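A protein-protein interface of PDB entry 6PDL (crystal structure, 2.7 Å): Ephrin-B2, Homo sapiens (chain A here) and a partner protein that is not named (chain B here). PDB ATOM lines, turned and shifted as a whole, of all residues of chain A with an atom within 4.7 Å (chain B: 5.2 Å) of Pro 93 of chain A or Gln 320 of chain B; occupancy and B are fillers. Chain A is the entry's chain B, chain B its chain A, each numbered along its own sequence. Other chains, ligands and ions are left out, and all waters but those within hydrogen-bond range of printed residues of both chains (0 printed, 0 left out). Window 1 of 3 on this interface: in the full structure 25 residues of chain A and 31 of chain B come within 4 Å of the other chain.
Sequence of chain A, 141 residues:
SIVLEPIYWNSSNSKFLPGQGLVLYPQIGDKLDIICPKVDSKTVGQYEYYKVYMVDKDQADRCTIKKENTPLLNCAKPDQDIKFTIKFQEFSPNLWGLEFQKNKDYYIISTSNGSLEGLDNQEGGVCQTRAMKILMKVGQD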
ATOM      1  N   PHE A  84     -23.403  -8.412 -18.401  1.00  0.00           N
ATOM      2  CA  PHE A  84     -22.269  -9.161 -18.912  1.00  0.00           C
ATOM      3  C   PHE A  84     -22.490 -10.623 -18.568  1.00  0.00           C
ATOM      4  O   PHE A  84     -22.698 -10.960 -17.398  1.00  0.00           O
ATOM      5  CB  PHE A  84     -20.956  -8.644 -18.318  1.00  0.00           C
ATOM      6  CG  PHE A  84     -19.758  -9.454 -18.708  1.00  0.00           C
ATOM      7  CD1 PHE A  84     -19.525  -9.771 -20.036  1.00  0.00           C
ATOM      8  CD2 PHE A  84     -18.866  -9.896 -17.752  1.00  0.00           C
ATOM      9  CE1 PHE A  84     -18.429 -10.514 -20.399  1.00  0.00           C
ATOM     10  CE2 PHE A  84     -17.764 -10.639 -18.109  1.00  0.00           C
ATOM     11  CZ  PHE A  84     -17.545 -10.950 -19.438  1.00  0.00           C
ATOM     12  N   SER A  92     -15.370 -17.768 -26.903  1.00  0.00           N
ATOM     13  CA  SER A  92     -15.865 -16.498 -26.394  1.00  0.00           C
ATOM     14  C   SER A  92     -15.865 -15.496 -27.533  1.00  0.00           C
ATOM     15  O   SER A  92     -15.037 -15.605 -28.444  1.00  0.00           O
ATOM     16  CB  SER A  92     -15.001 -15.985 -25.240  1.00  0.00           C
ATOM     17  OG  SER A  92     -15.335 -14.641 -24.961  1.00  0.00           O
ATOM     18  N   PRO A  93     -16.733 -14.486 -27.492  1.00  0.00           N
ATOM     19  CA  PRO A  93     -16.599 -13.351 -28.407  1.00  0.00           C
ATOM     20  C   PRO A  93     -15.521 -12.360 -28.005  1.00  0.00           C
ATOM     21  O   PRO A  93     -15.395 -11.317 -28.651  1.00  0.00           O
ATOM     22  CB  PRO A  93     -17.988 -12.689 -28.342  1.00  0.00           C
ATOM     23  CG  PRO A  93     -18.878 -13.685 -27.669  1.00  0.00           C
ATOM     24  CD  PRO A  93     -17.992 -14.429 -26.737  1.00  0.00           C
ATOM     25  N   ASN A  94     -14.768 -12.667 -26.954  1.00  0.00           N
ATOM     26  CA  ASN A  94     -13.661 -11.829 -26.520  1.00  0.00           C
ATOM     27  C   ASN A  94     -12.470 -12.020 -27.445  1.00  0.00           C
ATOM     28  O   ASN A  94     -12.026 -13.145 -27.679  1.00  0.00           O
ATOM     29  CB  ASN A  94     -13.265 -12.167 -25.086  1.00  0.00           C
ATOM     30  CG  ASN A  94     -12.348 -11.130 -24.478  1.00  0.00           C
ATOM     31  OD1 ASN A  94     -11.146 -11.103 -24.756  1.00  0.00           O
ATOM     32  ND2 ASN A  94     -12.913 -10.263 -23.647  1.00  0.00           N
ATOM     33  N   LEU A  95     -11.935 -10.915 -27.942  1.00  0.00           N
ATOM     34  CA  LEU A  95     -10.857 -10.966 -28.911  1.00  0.00           C
ATOM     35  C   LEU A  95      -9.488 -10.994 -28.250  1.00  0.00           C
ATOM     36  O   LEU A  95      -8.482 -11.192 -28.941  1.00  0.00           O
ATOM     37  CB  LEU A  95     -10.971  -9.776 -29.871  1.00  0.00           C
ATOM     38  CG  LEU A  95     -11.798  -9.999 -31.148  1.00  0.00           C
ATOM     39  CD1 LEU A  95     -13.023 -10.863 -30.906  1.00  0.00           C
ATOM     40  CD2 LEU A  95     -12.226  -8.665 -31.742  1.00  0.00           C
ATOM     41  N   LEU A  98     -10.309 -14.561 -23.719  1.00  0.00           N
ATOM     42  CA  LEU A  98     -10.962 -14.759 -22.432  1.00  0.00           C
ATOM     43  C   LEU A  98     -11.187 -16.248 -22.257  1.00  0.00           C
ATOM     44  O   LEU A  98     -11.997 -16.852 -22.967  1.00  0.00           O
ATOM     45  CB  LEU A  98     -12.293 -14.006 -22.392  1.00  0.00           C
ATOM     46  CG  LEU A  98     -13.407 -14.069 -21.330  1.00  0.00           C
ATOM     47  CD1 LEU A  98     -14.295 -12.874 -21.545  1.00  0.00           C
ATOM     48  CD2 LEU A  98     -14.268 -15.315 -21.407  1.00  0.00           C
ATOM     49  N   PRO B 318     -22.670 -12.613 -31.471  1.00  0.00           N
ATOM     50  CA  PRO B 318     -22.504 -12.378 -30.032  1.00  0.00           C
ATOM     51  C   PRO B 318     -21.368 -11.409 -29.752  1.00  0.00           C
ATOM     52  O   PRO B 318     -20.378 -11.343 -30.486  1.00  0.00           O
ATOM     53  CB  PRO B 318     -22.189 -13.771 -29.470  1.00  0.00           C
ATOM     54  CG  PRO B 318     -22.574 -14.734 -30.541  1.00  0.00           C
ATOM     55  CD  PRO B 318     -22.394 -14.013 -31.835  1.00  0.00           C
ATOM     56  N   GLY B 319     -21.505 -10.672 -28.655  1.00  0.00           N
ATOM     57  CA  GLY B 319     -20.497  -9.719 -28.252  1.00  0.00           C
ATOM     58  C   GLY B 319     -20.145  -9.852 -26.783  1.00  0.00           C
ATOM     59  O   GLY B 319     -20.204 -10.934 -26.189  1.00  0.00           O
ATOM     60  N   GLN B 320     -19.776  -8.718 -26.200  1.00  0.00           N
ATOM     61  CA  GLN B 320     -19.486  -8.616 -24.773  1.00  0.00           C
ATOM     62  C   GLN B 320     -20.372  -7.497 -24.237  1.00  0.00           C
ATOM     63  O   GLN B 320     -21.357  -7.093 -24.862  1.00  0.00           O
ATOM     64  CB  GLN B 320     -17.995  -8.392 -24.502  1.00  0.00           C
ATOM     65  CG  GLN B 320     -17.092  -9.463 -25.084  1.00  0.00           C
ATOM     66  CD  GLN B 320     -16.826 -10.596 -24.112  1.00  0.00           C
ATOM     67  OE1 GLN B 320     -15.798 -10.615 -23.431  1.00  0.00           O
ATOM     68  NE2 GLN B 320     -17.755 -11.545 -24.038  1.00  0.00           N
ATOM     69  N   SER B 321     -20.041  -7.003 -23.044  1.00  0.00           N
ATOM     70  CA  SER B 321     -20.908  -6.048 -22.355  1.00  0.00           C
ATOM     71  C   SER B 321     -21.215  -4.813 -23.196  1.00  0.00           C
ATOM     72  O   SER B 321     -22.376  -4.389 -23.287  1.00  0.00           O
ATOM     73  CB  SER B 321     -20.261  -5.654 -21.034  1.00  0.00           C
ATOM     74  OG  SER B 321     -20.981  -4.614 -20.413  1.00  0.00           O
ATOM     75  N   GLN B 322     -20.196  -4.231 -23.837  1.00  0.00           N
ATOM     76  CA  GLN B 322     -20.373  -2.915 -24.455  1.00  0.00           C
ATOM     77  C   GLN B 322     -21.141  -2.978 -25.771  1.00  0.00           C
ATOM     78  O   GLN B 322     -21.981  -2.109 -26.048  1.00  0.00           O
ATOM     79  CB  GLN B 322     -19.008  -2.262 -24.667  1.00  0.00           C
ATOM     80  CG  GLN B 322     -19.091  -0.800 -25.032  1.00  0.00           C
ATOM     81  CD  GLN B 322     -19.094   0.093 -23.813  1.00  0.00           C
ATOM     82  OE1 GLN B 322     -20.110   0.217 -23.127  1.00  0.00           O
ATOM     83  NE2 GLN B 322     -17.952   0.715 -23.529  1.00  0.00           N
ATOM     84  N   CYS B 323     -20.868  -3.979 -26.606  1.00  0.00           N
ATOM     85  CA  CYS B 323     -21.539  -4.132 -27.901  1.00  0.00           C
ATOM     86  C   CYS B 323     -21.949  -5.581 -28.094  1.00  0.00           C
ATOM     87  O   CYS B 323     -21.369  -6.304 -28.907  1.00  0.00           O
ATOM     88  CB  CYS B 323     -20.621  -3.683 -29.048  1.00  0.00           C
ATOM     89  SG  CYS B 323     -19.765  -2.122 -28.756  1.00  0.00           S
ATOM     90  N   PRO B 324     -22.967  -6.030 -27.387  1.00  0.00           N
ATOM     91  CA  PRO B 324     -23.456  -7.399 -27.558  1.00  0.00           C
ATOM     92  C   PRO B 324     -24.295  -7.485 -28.829  1.00  0.00           C
ATOM     93  O   PRO B 324     -24.426  -6.519 -29.587  1.00  0.00           O
ATOM     94  CB  PRO B 324     -24.287  -7.635 -26.298  1.00  0.00           C
ATOM     95  CG  PRO B 324     -24.828  -6.316 -25.957  1.00  0.00           C
ATOM     96  CD  PRO B 324     -23.764  -5.303 -26.377  1.00  0.00           C
ATOM     97  N   GLU B 335     -14.848  -6.574 -30.095  1.00  0.00           N
ATOM     98  CA  GLU B 335     -15.294  -7.912 -29.739  1.00  0.00           C
ATOM     99  C   GLU B 335     -16.208  -8.434 -30.834  1.00  0.00           C
ATOM    100  O   GLU B 335     -16.740  -7.667 -31.640  1.00  0.00           O
ATOM    101  CB  GLU B 335     -16.009  -7.927 -28.382  1.00  0.00           C
ATOM    102  CG  GLU B 335     -17.293  -7.111 -28.337  1.00  0.00           C
ATOM    103  CD  GLU B 335     -17.447  -6.322 -27.035  1.00  0.00           C
ATOM    104  OE1 GLU B 335     -16.414  -5.923 -26.447  1.00  0.00           O
ATOM    105  OE2 GLU B 335     -18.601  -6.104 -26.597  1.00  0.00           O
ATOM    106  N   GLY B 336     -16.360  -9.753 -30.871  1.00  0.00           N
ATOM    107  CA  GLY B 336     -17.255 -10.384 -31.812  1.00  0.00           C
ATOM    108  C   GLY B 336     -16.709 -11.708 -32.299  1.00  0.00           C
ATOM    109  O   GLY B 336     -15.726 -12.239 -31.783  1.00  0.00           O
ATOM    110  N   THR B 337     -17.391 -12.262 -33.298  1.00  0.00           N
ATOM    111  CA  THR B 337     -17.020 -13.527 -33.908  1.00  0.00           C
ATOM    112  C   THR B 337     -17.037 -13.369 -35.422  1.00  0.00           C
ATOM    113  O   THR B 337     -17.638 -12.438 -35.963  1.00  0.00           O
ATOM    114  CB  THR B 337     -17.976 -14.652 -33.491  1.00  0.00           C
ATOM    115  OG1 THR B 337     -19.217 -14.497 -34.186  1.00  0.00           O
ATOM    116  CG2 THR B 337     -18.242 -14.620 -31.985  1.00  0.00           C
ATOM    117  N   GLN B 360     -24.167 -12.870 -25.830  1.00  0.00           N
ATOM    118  CA  GLN B 360     -22.804 -12.576 -25.415  1.00  0.00           C
ATOM    119  C   GLN B 360     -21.929 -13.811 -25.285  1.00  0.00           C
ATOM    120  O   GLN B 360     -20.762 -13.678 -24.904  1.00  0.00           O
ATOM    121  CB  GLN B 360     -22.797 -11.817 -24.077  1.00  0.00           C
ATOM    122  CG  GLN B 360     -23.408 -10.433 -24.158  1.00  0.00           C
ATOM    123  CD  GLN B 360     -23.213  -9.623 -22.892  1.00  0.00           C
ATOM    124  OE1 GLN B 360     -22.091  -9.458 -22.410  1.00  0.00           O
ATOM    125  NE2 GLN B 360     -24.307  -9.106 -22.349  1.00  0.00           N
ATOM    126  N   THR B 361     -22.447 -14.996 -25.587  1.00  0.00           N
ATOM    127  CA  THR B 361     -21.700 -16.236 -25.438  1.00  0.00           C
ATOM    128  C   THR B 361     -21.523 -16.903 -26.796  1.00  0.00           C
ATOM    129  O   THR B 361     -22.349 -16.748 -27.700  1.00  0.00           O
ATOM    130  CB  THR B 361     -22.388 -17.196 -24.465  1.00  0.00           C
ATOM    131  OG1 THR B 361     -23.773 -17.307 -24.804  1.00  0.00           O
ATOM    132  CG2 THR B 361     -22.261 -16.688 -23.043  1.00  0.00           C
ATOM    133  N   ALA B 362     -20.419 -17.632 -26.939  1.00  0.00           N
ATOM    134  CA  ALA B 362     -20.121 -18.368 -28.169  1.00  0.00           C
ATOM    135  C   ALA B 362     -20.758 -19.757 -28.113  1.00  0.00           C
ATOM    136  O   ALA B 362     -20.103 -20.765 -27.836  1.00  0.00           O
ATOM    137  CB  ALA B 362     -18.612 -18.443 -28.370  1.00  0.00           C
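OE1 of Gln 320 of chain B sits at hydrogen-bond distance from ND2 of Asn 94 of chain A, 2.9 Å away. The backbone NH (N) of Gly 336 of chain B is in hydrogen-bond range of the backbone carbonyl oxygen (O) of Pro 93 of chain A, at 2.9 Å.
The side-chain carboxylate of Glu 335 of chain B sits at hydrogen-bond distance from the backbone NH of Gln 320 of chain B (2.9 Å). The backbone carbonyl oxygen (O) of Gln 320 of chain B sits close to the side-chain amide oxygen (OE1) of Gln 360 of chain B (3.5 Å). The side-chain amide oxygen (OE1) of Gln 360 of chain B sits at hydrogen-bond distance from the backbone NH (N) of Ser 321 of chain B, 3.3 Å away. OE2 of Glu 335 of chain B lies within hydrogen-bond range of N of Cys 323 of chain B. The side-chain hydroxyl (OG) of Ser 92 of chain A sits at hydrogen-bond distance from the backbone NH (N) of Asn 94 of chain A, 2.9 Å away.
Among the printed residues, pairs that only touch across the chains: Leu 95 of chain A with Gly 336 of chain B, Leu 98 of chain A with Gln 320 of chain B, Pro 93 of chain A with Gln 360 of chain B, Pro 93 of chain A with Gly 319 of chain B, Pro 93 of chain A with Glu 335 of chain B, Pro 93 of chain A with Pro 318 of chain B, Phe 84 of chain A with Gln 360 of chain B, Ser 92 of chain A with Ala 362 of chain B, Leu 95 of chain A with Glu 335 of chain B, Phe 84 of chain A with Gln 320 of chain B and Pro 93 of chain A with Gln 320 of chain B.
Of the printed residues of chain B, Pro 93 of chain A touches Pro 318, Gly 319, Gln 320, Glu 335, Gly 336 and Gln 360. Printed residues of chain A within 4 Å of Gln 320 of chain B: Phe 84 (3.8 Å), Pro 93 (3.96 Å), Asn 94 (2.9 Å) and Leu 98 (3.3 Å). Printed residues of chain B within 4 Å of Asn 94 of chain A: Gln 320 (2.9 Å). Of the printed residues of chain A, Glu 335 of chain B touches Pro 93 and Leu 95. Of the printed residues of chain A, Gly 319 of chain B touches Pro 93 (3.4 Å). Of the printed residues of chain A, Gln 360 of chain B touches Phe 84 (3.5 Å) and Pro 93 (3.3 Å). Ser 321 of chain B touches none of the printed residues of chain A. Thr 337 of chain B touches none of the printed residues of chain A. The nearest printed residue of chain A that does not touch Glu 335 of chain B is Asn 94 of chain A (4.9 Å).
Printed residues of chain A that touch a printed residue of chain B: Phe 84, Ser 92, Pro 93, Asn 94, Leu 95 and Leu 98. Hydrophobic or aromatic side chains of chain A within 4 Å of the printed part of chain B: Phe 84, Pro 93, Leu 95 and Leu 98. Along chain A the printed residues that touch a printed residue of chain B span positions 84 to 98. Among the printed residues, no Asp or Glu carboxylate lies within 4 Å of a Lys or Arg side-chain nitrogen of the other chain.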
